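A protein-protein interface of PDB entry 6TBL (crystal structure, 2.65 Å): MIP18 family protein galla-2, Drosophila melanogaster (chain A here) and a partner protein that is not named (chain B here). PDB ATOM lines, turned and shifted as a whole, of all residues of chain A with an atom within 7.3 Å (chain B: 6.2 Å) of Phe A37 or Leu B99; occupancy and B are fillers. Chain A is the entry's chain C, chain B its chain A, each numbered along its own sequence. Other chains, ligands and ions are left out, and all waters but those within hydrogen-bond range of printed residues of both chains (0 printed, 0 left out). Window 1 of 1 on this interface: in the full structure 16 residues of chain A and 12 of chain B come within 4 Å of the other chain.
The side-chain carboxylate of Glu A41 lies within salt-bridge range of the guanidinium group of Arg B107 (2.6 Å).
The backbone carbonyl oxygen of Arg A105 sits at hydrogen-bond distance from the guanidinium group of Arg B114, 2.7 Å away.
The backbone carbonyl oxygen of Asp A35 lies close to the guanidinium group of Arg B107, 2.4 Å away.
The side-chain carboxylate (OD2) of Asp B100 is in salt-bridge range of the guanidinium group (NE) of Arg A110.
N of Phe A37 is in hydrogen-bond range of OD2 of Asp A73 (3.2 Å).
N of Glu A41 lies within hydrogen-bond range of OD1 of Asp A38, at 3.3 Å.
O of Asp B101 lies within hydrogen-bond range of NE of Arg B107 (2.9 Å).
The side-chain carboxylate (OD1) of Asp A73 is in salt-bridge range of the guanidinium group (NH1) of Arg A110, at 2.5 Å.
Among the printed residues, pairs that only touch across the chains: Phe A37 with Arg B107, Ser A106 with Val B111, Arg A105 with Leu B99, Pro A108 with Leu B99, Ser A106 with Leu B99, Phe A37 with Leu B99, Pro A108 with Asp B100, Phe A37 with Asp B100, Leu A107 with Leu B99, Leu A45 with Val B111 and Pro A36 with Arg B107.
Leu B99 touches just these residues of chain A: Phe A37 (3.5 Å), Arg A105 (3.5 Å), Ser A106 (3.5 Å), Leu A107 (3.8 Å) and Pro A108 (3.5 Å).
Of the printed residues of chain A, Asp B100 touches Phe A37 (3.7 Å), Pro A108 (3.6 Å) and Arg A110 (2.9 Å).
Printed residues of chain B within 4 Å of Pro A108: Leu B99 and Asp B100.
Printed residues of chain B within 4 Å of Ser A106: Leu B99 (3.5 Å) and Val B111 (3.4 Å).
Leu A103 touches none of the printed residues of chain B.
Ala B96 touches none of the printed residues of chain A.
The nearest residue of chain A that does not touch Leu B99 is Glu A41 (5.8 Å).
Of the 12 printed residues of chain B, 5 touch a printed residue of chain A.
Hydrophobic or aromatic side chains of chain B that line the printed part of chain A: Leu B99 and Val B111.
Of the 23 printed residues of chain A, 10 touch a printed residue of chain B.
Hydrophobic or aromatic side chains of chain A that line the printed part of chain B: Phe A37, Leu A45 and Pro A108.
Among the printed residues, 15 pairs touch across the chains.
Among the printed residues, Asp or Glu carboxylates within 4 Å of a Lys or Arg side-chain nitrogen of the other chain: Glu A41 with Arg B107 (2.6 Å) and Arg A110 with Asp B100 (2.9 Å).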
ATOM      1  N   ASP A  35      27.038  12.083 -10.268  1.00  0.00           N
ATOM      2  CA  ASP A  35      26.125  11.258  -9.482  1.00  0.00           C
ATOM      3  C   ASP A  35      26.309   9.794  -9.852  1.00  0.00           C
ATOM      4  O   ASP A  35      25.993   9.404 -10.987  1.00  0.00           O
ATOM      5  CB  ASP A  35      24.675  11.686  -9.712  1.00  0.00           C
ATOM      6  CG  ASP A  35      24.388  13.079  -9.187  1.00  0.00           C
ATOM      7  OD1 ASP A  35      25.086  13.516  -8.246  1.00  0.00           O
ATOM      8  OD2 ASP A  35      23.461  13.736  -9.712  1.00  0.00           O
ATOM      9  N   PRO A  36      26.806   8.951  -8.952  1.00  0.00           N
ATOM     10  CA  PRO A  36      27.024   7.545  -9.307  1.00  0.00           C
ATOM     11  C   PRO A  36      25.720   6.779  -9.455  1.00  0.00           C
ATOM     12  O   PRO A  36      24.693   7.129  -8.870  1.00  0.00           O
ATOM     13  CB  PRO A  36      27.849   7.008  -8.131  1.00  0.00           C
ATOM     14  CG  PRO A  36      27.482   7.895  -6.987  1.00  0.00           C
ATOM     15  CD  PRO A  36      27.261   9.256  -7.584  1.00  0.00           C
ATOM     16  N   PHE A  37      25.775   5.726 -10.268  1.00  0.00           N
ATOM     17  CA  PHE A  37      24.672   4.782 -10.354  1.00  0.00           C
ATOM     18  C   PHE A  37      24.558   4.021  -9.040  1.00  0.00           C
ATOM     19  O   PHE A  37      25.563   3.591  -8.470  1.00  0.00           O
ATOM     20  CB  PHE A  37      24.891   3.797 -11.504  1.00  0.00           C
ATOM     21  CG  PHE A  37      24.625   4.369 -12.871  1.00  0.00           C
ATOM     22  CD1 PHE A  37      23.429   4.110 -13.525  1.00  0.00           C
ATOM     23  CD2 PHE A  37      25.576   5.145 -13.515  1.00  0.00           C
ATOM     24  CE1 PHE A  37      23.183   4.624 -14.790  1.00  0.00           C
ATOM     25  CE2 PHE A  37      25.334   5.665 -14.781  1.00  0.00           C
ATOM     26  CZ  PHE A  37      24.137   5.403 -15.416  1.00  0.00           C
ATOM     27  N   ASP A  38      23.330   3.852  -8.558  1.00  0.00           N
ATOM     28  CA  ASP A  38      23.099   3.184  -7.288  1.00  0.00           C
ATOM     29  C   ASP A  38      21.932   2.217  -7.428  1.00  0.00           C
ATOM     30  O   ASP A  38      21.274   2.143  -8.471  1.00  0.00           O
ATOM     31  CB  ASP A  38      22.846   4.194  -6.161  1.00  0.00           C
ATOM     32  CG  ASP A  38      21.629   5.058  -6.415  1.00  0.00           C
ATOM     33  OD1 ASP A  38      21.274   5.270  -7.593  1.00  0.00           O
ATOM     34  OD2 ASP A  38      21.027   5.527  -5.428  1.00  0.00           O
ATOM     35  N   LYS A  39      21.691   1.459  -6.355  1.00  0.00           N
ATOM     36  CA  LYS A  39      20.622   0.465  -6.364  1.00  0.00           C
ATOM     37  C   LYS A  39      19.271   1.111  -6.626  1.00  0.00           C
ATOM     38  O   LYS A  39      18.424   0.540  -7.323  1.00  0.00           O
ATOM     39  CB  LYS A  39      20.598  -0.287  -5.033  1.00  0.00           C
ATOM     40  CG  LYS A  39      21.901  -0.978  -4.668  1.00  0.00           C
ATOM     41  CD  LYS A  39      21.947  -1.318  -3.182  1.00  0.00           C
ATOM     42  CE  LYS A  39      20.788  -2.210  -2.766  1.00  0.00           C
ATOM     43  NZ  LYS A  39      20.793  -2.469  -1.295  1.00  0.00           N
ATOM     44  N   ARG A  40      19.052   2.302  -6.069  1.00  0.00           N
ATOM     45  CA  ARG A  40      17.764   2.966  -6.225  1.00  0.00           C
ATOM     46  C   ARG A  40      17.480   3.284  -7.684  1.00  0.00           C
ATOM     47  O   ARG A  40      16.358   3.082  -8.167  1.00  0.00           O
ATOM     48  CB  ARG A  40      17.731   4.238  -5.383  1.00  0.00           C
ATOM     49  CG  ARG A  40      16.459   5.042  -5.526  1.00  0.00           C
ATOM     50  CD  ARG A  40      15.258   4.262  -5.023  1.00  0.00           C
ATOM     51  NE  ARG A  40      14.036   5.054  -5.104  1.00  0.00           N
ATOM     52  CZ  ARG A  40      13.622   5.885  -4.153  1.00  0.00           C
ATOM     53  NH1 ARG A  40      14.334   6.034  -3.043  1.00  0.00           N
ATOM     54  NH2 ARG A  40      12.498   6.570  -4.314  1.00  0.00           N
ATOM     55  N   GLU A  41      18.486   3.779  -8.406  1.00  0.00           N
ATOM     56  CA  GLU A  41      18.275   4.167  -9.795  1.00  0.00           C
ATOM     57  C   GLU A  41      17.932   2.960 -10.656  1.00  0.00           C
ATOM     58  O   GLU A  41      17.035   3.027 -11.505  1.00  0.00           O
ATOM     59  CB  GLU A  41      19.518   4.881 -10.321  1.00  0.00           C
ATOM     60  CG  GLU A  41      19.370   5.469 -11.702  1.00  0.00           C
ATOM     61  CD  GLU A  41      20.589   6.267 -12.103  1.00  0.00           C
ATOM     62  OE1 GLU A  41      21.484   6.444 -11.251  1.00  0.00           O
ATOM     63  OE2 GLU A  41      20.659   6.717 -13.267  1.00  0.00           O
ATOM     64  N   ILE A  42      18.626   1.842 -10.439  1.00  0.00           N
ATOM     65  CA  ILE A  42      18.310   0.623 -11.172  1.00  0.00           C
ATOM     66  C   ILE A  42      16.931   0.111 -10.777  1.00  0.00           C
ATOM     67  O   ILE A  42      16.153  -0.341 -11.627  1.00  0.00           O
ATOM     68  CB  ILE A  42      19.402  -0.435 -10.936  1.00  0.00           C
ATOM     69  CG1 ILE A  42      20.755   0.092 -11.408  1.00  0.00           C
ATOM     70  CG2 ILE A  42      19.066  -1.724 -11.661  1.00  0.00           C
ATOM     71  CD1 ILE A  42      20.807   0.376 -12.894  1.00  0.00           C
ATOM     72  N   LEU A  45      14.252   1.663 -12.545  1.00  0.00           N
ATOM     73  CA  LEU A  45      14.168   1.269 -13.945  1.00  0.00           C
ATOM     74  C   LEU A  45      13.331   0.017 -14.157  1.00  0.00           C
ATOM     75  O   LEU A  45      12.797  -0.175 -15.254  1.00  0.00           O
ATOM     76  CB  LEU A  45      15.569   1.050 -14.512  1.00  0.00           C
ATOM     77  CG  LEU A  45      16.387   2.318 -14.745  1.00  0.00           C
ATOM     78  CD1 LEU A  45      17.823   1.964 -15.050  1.00  0.00           C
ATOM     79  CD2 LEU A  45      15.781   3.125 -15.882  1.00  0.00           C
ATOM     80  N   ILE A  71      25.060  -3.427  -7.703  1.00  0.00           N
ATOM     81  CA  ILE A  71      25.638  -2.617  -8.769  1.00  0.00           C
ATOM     82  C   ILE A  71      26.915  -1.969  -8.256  1.00  0.00           C
ATOM     83  O   ILE A  71      27.014  -1.599  -7.083  1.00  0.00           O
ATOM     84  CB  ILE A  71      24.635  -1.555  -9.277  1.00  0.00           C
ATOM     85  CG1 ILE A  71      25.245  -0.741 -10.419  1.00  0.00           C
ATOM     86  CG2 ILE A  71      24.191  -0.641  -8.140  1.00  0.00           C
ATOM     87  CD1 ILE A  71      24.326   0.304 -10.980  1.00  0.00           C
ATOM     88  N   ASN A  72      27.905  -1.863  -9.140  1.00  0.00           N
ATOM     89  CA  ASN A  72      29.111  -1.082  -8.894  1.00  0.00           C
ATOM     90  C   ASN A  72      29.329  -0.204 -10.118  1.00  0.00           C
ATOM     91  O   ASN A  72      29.654  -0.708 -11.198  1.00  0.00           O
ATOM     92  CB  ASN A  72      30.322  -1.975  -8.632  1.00  0.00           C
ATOM     93  CG  ASN A  72      31.521  -1.196  -8.127  1.00  0.00           C
ATOM     94  OD1 ASN A  72      32.140  -0.434  -8.871  1.00  0.00           O
ATOM     95  ND2 ASN A  72      31.860  -1.390  -6.861  1.00  0.00           N
ATOM     96  N   ASP A  73      29.128   1.103  -9.948  1.00  0.00           N
ATOM     97  CA  ASP A  73      29.272   2.031 -11.064  1.00  0.00           C
ATOM     98  C   ASP A  73      30.683   1.978 -11.638  1.00  0.00           C
ATOM     99  O   ASP A  73      30.867   1.899 -12.858  1.00  0.00           O
ATOM    100  CB  ASP A  73      28.919   3.447 -10.601  1.00  0.00           C
ATOM    101  CG  ASP A  73      28.841   4.439 -11.744  1.00  0.00           C
ATOM    102  OD1 ASP A  73      28.912   4.023 -12.919  1.00  0.00           O
ATOM    103  OD2 ASP A  73      28.704   5.649 -11.459  1.00  0.00           O
ATOM    104  N   SER A  74      31.695   2.002 -10.768  1.00  0.00           N
ATOM    105  CA  SER A  74      33.073   2.046 -11.246  1.00  0.00           C
ATOM    106  C   SER A  74      33.452   0.761 -11.970  1.00  0.00           C
ATOM    107  O   SER A  74      34.126   0.801 -13.007  1.00  0.00           O
ATOM    108  CB  SER A  74      34.021   2.309 -10.078  1.00  0.00           C
ATOM    109  OG  SER A  74      35.364   2.356 -10.523  1.00  0.00           O
ATOM    110  N   VAL A  78      26.283  -4.725 -13.084  1.00  0.00           N
ATOM    111  CA  VAL A  78      24.941  -4.702 -12.512  1.00  0.00           C
ATOM    112  C   VAL A  78      24.457  -6.137 -12.390  1.00  0.00           C
ATOM    113  O   VAL A  78      24.540  -6.908 -13.352  1.00  0.00           O
ATOM    114  CB  VAL A  78      23.952  -3.879 -13.361  1.00  0.00           C
ATOM    115  CG1 VAL A  78      22.563  -3.915 -12.731  1.00  0.00           C
ATOM    116  CG2 VAL A  78      24.435  -2.452 -13.508  1.00  0.00           C
ATOM    117  N   LEU A 103      16.752  -2.689 -19.201  1.00  0.00           N
ATOM    118  CA  LEU A 103      18.100  -2.278 -18.826  1.00  0.00           C
ATOM    119  C   LEU A 103      19.004  -2.137 -20.043  1.00  0.00           C
ATOM    120  O   LEU A 103      19.865  -1.251 -20.073  1.00  0.00           O
ATOM    121  CB  LEU A 103      18.691  -3.267 -17.822  1.00  0.00           C
ATOM    122  CG  LEU A 103      17.954  -3.319 -16.485  1.00  0.00           C
ATOM    123  CD1 LEU A 103      18.628  -4.299 -15.541  1.00  0.00           C
ATOM    124  CD2 LEU A 103      17.888  -1.930 -15.863  1.00  0.00           C
ATOM    125  N   LEU A 104      18.818  -2.988 -21.056  1.00  0.00           N
ATOM    126  CA  LEU A 104      19.614  -2.869 -22.273  1.00  0.00           C
ATOM    127  C   LEU A 104      19.379  -1.532 -22.964  1.00  0.00           C
ATOM    128  O   LEU A 104      20.307  -0.956 -23.543  1.00  0.00           O
ATOM    129  CB  LEU A 104      19.295  -4.026 -23.221  1.00  0.00           C
ATOM    130  CG  LEU A 104      20.006  -4.072 -24.574  1.00  0.00           C
ATOM    131  CD1 LEU A 104      21.513  -4.174 -24.390  1.00  0.00           C
ATOM    132  CD2 LEU A 104      19.482  -5.231 -25.410  1.00  0.00           C
ATOM    133  N   ARG A 105      18.153  -1.017 -22.904  1.00  0.00           N
ATOM    134  CA  ARG A 105      17.830   0.258 -23.530  1.00  0.00           C
ATOM    135  C   ARG A 105      18.145   1.450 -22.641  1.00  0.00           C
ATOM    136  O   ARG A 105      18.478   2.525 -23.157  1.00  0.00           O
ATOM    137  CB  ARG A 105      16.347   0.297 -23.914  1.00  0.00           C
ATOM    138  CG  ARG A 105      15.935  -0.756 -24.931  1.00  0.00           C
ATOM    139  CD  ARG A 105      14.438  -0.719 -25.195  1.00  0.00           C
ATOM    140  NE  ARG A 105      14.030  -1.728 -26.170  1.00  0.00           N
ATOM    141  CZ  ARG A 105      12.773  -1.941 -26.549  1.00  0.00           C
ATOM    142  NH1 ARG A 105      11.788  -1.214 -26.040  1.00  0.00           N
ATOM    143  NH2 ARG A 105      12.503  -2.883 -27.442  1.00  0.00           N
ATOM    144  N   SER A 106      18.057   1.284 -21.321  1.00  0.00           N
ATOM    145  CA  SER A 106      18.170   2.399 -20.390  1.00  0.00           C
ATOM    146  C   SER A 106      19.575   2.606 -19.840  1.00  0.00           C
ATOM    147  O   SER A 106      19.879   3.708 -19.367  1.00  0.00           O
ATOM    148  CB  SER A 106      17.206   2.199 -19.217  1.00  0.00           C
ATOM    149  OG  SER A 106      15.909   1.864 -19.678  1.00  0.00           O
ATOM    150  N   LEU A 107      20.445   1.578 -19.887  1.00  0.00           N
ATOM    151  CA  LEU A 107      21.759   1.733 -19.284  1.00  0.00           C
ATOM    152  C   LEU A 107      22.821   1.984 -20.346  1.00  0.00           C
ATOM    153  O   LEU A 107      22.671   1.567 -21.496  1.00  0.00           O
ATOM    154  CB  LEU A 107      22.142   0.486 -18.481  1.00  0.00           C
ATOM    155  CG  LEU A 107      21.313   0.214 -17.229  1.00  0.00           C
ATOM    156  CD1 LEU A 107      21.896  -0.957 -16.455  1.00  0.00           C
ATOM    157  CD2 LEU A 107      21.261   1.462 -16.364  1.00  0.00           C
ATOM    158  N   PRO A 108      23.900   2.673 -19.979  1.00  0.00           N
ATOM    159  CA  PRO A 108      25.015   2.828 -20.907  1.00  0.00           C
ATOM    160  C   PRO A 108      25.591   1.471 -21.275  1.00  0.00           C
ATOM    161  O   PRO A 108      25.607   0.544 -20.447  1.00  0.00           O
ATOM    162  CB  PRO A 108      26.022   3.668 -20.111  1.00  0.00           C
ATOM    163  CG  PRO A 108      25.186   4.383 -19.108  1.00  0.00           C
ATOM    164  CD  PRO A 108      24.100   3.437 -18.738  1.00  0.00           C
ATOM    165  N   PRO A 109      26.082   1.317 -22.507  1.00  0.00           N
ATOM    166  CA  PRO A 109      26.566  -0.006 -22.938  1.00  0.00           C
ATOM    167  C   PRO A 109      27.767  -0.509 -22.153  1.00  0.00           C
ATOM    168  O   PRO A 109      28.055  -1.712 -22.198  1.00  0.00           O
ATOM    169  CB  PRO A 109      26.913   0.214 -24.416  1.00  0.00           C
ATOM    170  CG  PRO A 109      27.186   1.675 -24.519  1.00  0.00           C
ATOM    171  CD  PRO A 109      26.245   2.334 -23.557  1.00  0.00           C
ATOM    172  N   ARG A 110      28.468   0.364 -21.426  1.00  0.00           N
ATOM    173  CA  ARG A 110      29.591  -0.077 -20.606  1.00  0.00           C
ATOM    174  C   ARG A 110      29.159  -1.011 -19.485  1.00  0.00           C
ATOM    175  O   ARG A 110      29.999  -1.735 -18.941  1.00  0.00           O
ATOM    176  CB  ARG A 110      30.313   1.134 -20.010  1.00  0.00           C
ATOM    177  CG  ARG A 110      29.461   1.930 -19.045  1.00  0.00           C
ATOM    178  CD  ARG A 110      30.154   3.200 -18.595  1.00  0.00           C
ATOM    179  NE  ARG A 110      29.400   3.875 -17.543  1.00  0.00           N
ATOM    180  CZ  ARG A 110      29.569   3.644 -16.246  1.00  0.00           C
ATOM    181  NH1 ARG A 110      28.844   4.299 -15.354  1.00  0.00           N
ATOM    182  NH2 ARG A 110      30.468   2.760 -15.840  1.00  0.00           N
ATOM    183  N   PHE A 111      27.877  -1.014 -19.131  1.00  0.00           N
ATOM    184  CA  PHE A 111      27.383  -1.829 -18.030  1.00  0.00           C
ATOM    185  C   PHE A 111      27.098  -3.249 -18.495  1.00  0.00           C
ATOM    186  O   PHE A 111      26.379  -3.462 -19.477  1.00  0.00           O
ATOM    187  CB  PHE A 111      26.122  -1.206 -17.432  1.00  0.00           C
ATOM    188  CG  PHE A 111      26.396  -0.188 -16.366  1.00  0.00           C
ATOM    189  CD1 PHE A 111      26.858  -0.581 -15.120  1.00  0.00           C
ATOM    190  CD2 PHE A 111      26.190   1.161 -16.603  1.00  0.00           C
ATOM    191  CE1 PHE A 111      27.105   0.349 -14.127  1.00  0.00           C
ATOM    192  CE2 PHE A 111      26.436   2.101 -15.615  1.00  0.00           C
ATOM    193  CZ  PHE A 111      26.894   1.694 -14.376  1.00  0.00           C
ATOM    194  N   LEU B  95      21.602   9.067 -28.220  1.00  0.00           N
ATOM    195  CA  LEU B  95      21.057   9.148 -26.870  1.00  0.00           C
ATOM    196  C   LEU B  95      21.742   8.199 -25.896  1.00  0.00           C
ATOM    197  O   LEU B  95      21.453   8.261 -24.696  1.00  0.00           O
ATOM    198  CB  LEU B  95      19.548   8.880 -26.890  1.00  0.00           C
ATOM    199  CG  LEU B  95      18.707   9.972 -27.556  1.00  0.00           C
ATOM    200  CD1 LEU B  95      17.224   9.664 -27.461  1.00  0.00           C
ATOM    201  CD2 LEU B  95      19.012  11.325 -26.941  1.00  0.00           C
ATOM    202  N   ALA B  96      22.638   7.332 -26.371  1.00  0.00           N
ATOM    203  CA  ALA B  96      23.386   6.482 -25.452  1.00  0.00           C
ATOM    204  C   ALA B  96      24.353   7.295 -24.601  1.00  0.00           C
ATOM    205  O   ALA B  96      24.638   6.919 -23.459  1.00  0.00           O
ATOM    206  CB  ALA B  96      24.137   5.401 -26.229  1.00  0.00           C
ATOM    207  N   LYS B  97      24.865   8.408 -25.135  1.00  0.00           N
ATOM    208  CA  LYS B  97      25.791   9.228 -24.355  1.00  0.00           C
ATOM    209  C   LYS B  97      25.105   9.896 -23.170  1.00  0.00           C
ATOM    210  O   LYS B  97      25.637   9.804 -22.049  1.00  0.00           O
ATOM    211  CB  LYS B  97      26.485  10.242 -25.270  1.00  0.00           C
ATOM    212  CG  LYS B  97      27.348  11.256 -24.539  1.00  0.00           C
ATOM    213  CD  LYS B  97      27.878  12.315 -25.498  1.00  0.00           C
ATOM    214  CE  LYS B  97      28.730  13.343 -24.775  1.00  0.00           C
ATOM    215  NZ  LYS B  97      29.239  14.389 -25.702  1.00  0.00           N
ATOM    216  N   PRO B  98      23.953  10.565 -23.318  1.00  0.00           N
ATOM    217  CA  PRO B  98      23.283  11.127 -22.133  1.00  0.00           C
ATOM    218  C   PRO B  98      22.835  10.083 -21.126  1.00  0.00           C
ATOM    219  O   PRO B  98      22.532  10.446 -19.982  1.00  0.00           O
ATOM    220  CB  PRO B  98      22.081  11.875 -22.727  1.00  0.00           C
ATOM    221  CG  PRO B  98      22.471  12.172 -24.116  1.00  0.00           C
ATOM    222  CD  PRO B  98      23.277  10.990 -24.557  1.00  0.00           C
ATOM    223  N   LEU B  99      22.772   8.804 -21.509  1.00  0.00           N
ATOM    224  CA  LEU B  99      22.473   7.763 -20.531  1.00  0.00           C
ATOM    225  C   LEU B  99      23.566   7.657 -19.479  1.00  0.00           C
ATOM    226  O   LEU B  99      23.305   7.202 -18.360  1.00  0.00           O
ATOM    227  CB  LEU B  99      22.288   6.408 -21.218  1.00  0.00           C
ATOM    228  CG  LEU B  99      21.077   6.212 -22.132  1.00  0.00           C
ATOM    229  CD1 LEU B  99      21.037   4.782 -22.628  1.00  0.00           C
ATOM    230  CD2 LEU B  99      19.789   6.558 -21.409  1.00  0.00           C
ATOM    231  N   ASP B 100      24.790   8.060 -19.818  1.00  0.00           N
ATOM    232  CA  ASP B 100      25.918   8.032 -18.898  1.00  0.00           C
ATOM    233  C   ASP B 100      26.296   9.425 -18.406  1.00  0.00           C
ATOM    234  O   ASP B 100      27.446   9.652 -18.013  1.00  0.00           O
ATOM    235  CB  ASP B 100      27.119   7.360 -19.562  1.00  0.00           C
ATOM    236  CG  ASP B 100      28.081   6.769 -18.559  1.00  0.00           C
ATOM    237  OD1 ASP B 100      27.704   6.665 -17.373  1.00  0.00           O
ATOM    238  OD2 ASP B 100      29.212   6.416 -18.951  1.00  0.00           O
ATOM    239  N   ASP B 101      25.355  10.365 -18.428  1.00  0.00           N
ATOM    240  CA  ASP B 101      25.642  11.713 -17.968  1.00  0.00           C
ATOM    241  C   ASP B 101      25.903  11.718 -16.465  1.00  0.00           C
ATOM    242  O   ASP B 101      25.452  10.842 -15.723  1.00  0.00           O
ATOM    243  CB  ASP B 101      24.488  12.657 -18.301  1.00  0.00           C
ATOM    244  CG  ASP B 101      24.868  14.114 -18.140  1.00  0.00           C
ATOM    245  OD1 ASP B 101      25.118  14.783 -19.164  1.00  0.00           O
ATOM    246  OD2 ASP B 101      24.940  14.589 -16.987  1.00  0.00           O
ATOM    247  N   ARG B 107      20.031  11.948 -16.777  1.00  0.00           N
ATOM    248  CA  ARG B 107      19.973  10.551 -17.195  1.00  0.00           C
ATOM    249  C   ARG B 107      18.536  10.052 -17.253  1.00  0.00           C
ATOM    250  O   ARG B 107      18.164   9.318 -18.175  1.00  0.00           O
ATOM    251  CB  ARG B 107      20.798   9.682 -16.250  1.00  0.00           C
ATOM    252  CG  ARG B 107      22.292   9.718 -16.504  1.00  0.00           C
ATOM    253  CD  ARG B 107      22.997   8.733 -15.593  1.00  0.00           C
ATOM    254  NE  ARG B 107      23.423   9.355 -14.347  1.00  0.00           N
ATOM    255  CZ  ARG B 107      23.505   8.711 -13.190  1.00  0.00           C
ATOM    256  NH1 ARG B 107      23.174   7.434 -13.120  1.00  0.00           N
ATOM    257  NH2 ARG B 107      23.908   9.347 -12.103  1.00  0.00           N
ATOM    258  N   ALA B 110      17.131  11.091 -20.413  1.00  0.00           N
ATOM    259  CA  ALA B 110      17.721  10.328 -21.508  1.00  0.00           C
ATOM    260  C   ALA B 110      17.095   8.943 -21.614  1.00  0.00           C
ATOM    261  O   ALA B 110      16.818   8.462 -22.720  1.00  0.00           O
ATOM    262  CB  ALA B 110      19.233  10.225 -21.321  1.00  0.00           C
ATOM    263  N   VAL B 111      16.866   8.287 -20.476  1.00  0.00           N
ATOM    264  CA  VAL B 111      16.171   7.001 -20.480  1.00  0.00           C
ATOM    265  C   VAL B 111      14.780   7.156 -21.079  1.00  0.00           C
ATOM    266  O   VAL B 111      14.349   6.355 -21.918  1.00  0.00           O
ATOM    267  CB  VAL B 111      16.110   6.420 -19.055  1.00  0.00           C
ATOM    268  CG1 VAL B 111      15.177   5.224 -19.007  1.00  0.00           C
ATOM    269  CG2 VAL B 111      17.499   6.033 -18.588  1.00  0.00           C
ATOM    270  N   SER B 112      14.060   8.198 -20.661  1.00  0.00           N
ATOM    271  CA  SER B 112      12.700   8.402 -21.143  1.00  0.00           C
ATOM    272  C   SER B 112      12.673   8.688 -22.640  1.00  0.00           C
ATOM    273  O   SER B 112      11.831   8.150 -23.368  1.00  0.00           O
ATOM    274  CB  SER B 112      12.041   9.540 -20.364  1.00  0.00           C
ATOM    275  OG  SER B 112      10.726   9.787 -20.829  1.00  0.00           O
ATOM    276  N   ARG B 114      15.105   8.009 -24.999  1.00  0.00           N
ATOM    277  CA  ARG B 114      15.599   6.883 -25.784  1.00  0.00           C
ATOM    278  C   ARG B 114      14.599   5.735 -25.798  1.00  0.00           C
ATOM    279  O   ARG B 114      14.453   5.046 -26.814  1.00  0.00           O
ATOM    280  CB  ARG B 114      16.949   6.423 -25.234  1.00  0.00           C
ATOM    281  CG  ARG B 114      17.722   5.454 -26.118  1.00  0.00           C
ATOM    282  CD  ARG B 114      19.134   5.309 -25.581  1.00  0.00           C
ATOM    283  NE  ARG B 114      20.042   4.622 -26.495  1.00  0.00           N
ATOM    284  CZ  ARG B 114      20.528   3.403 -26.289  1.00  0.00           C
ATOM    285  NH1 ARG B 114      20.194   2.728 -25.198  1.00  0.00           N
ATOM    286  NH2 ARG B 114      21.352   2.860 -27.173  1.00  0.00           N
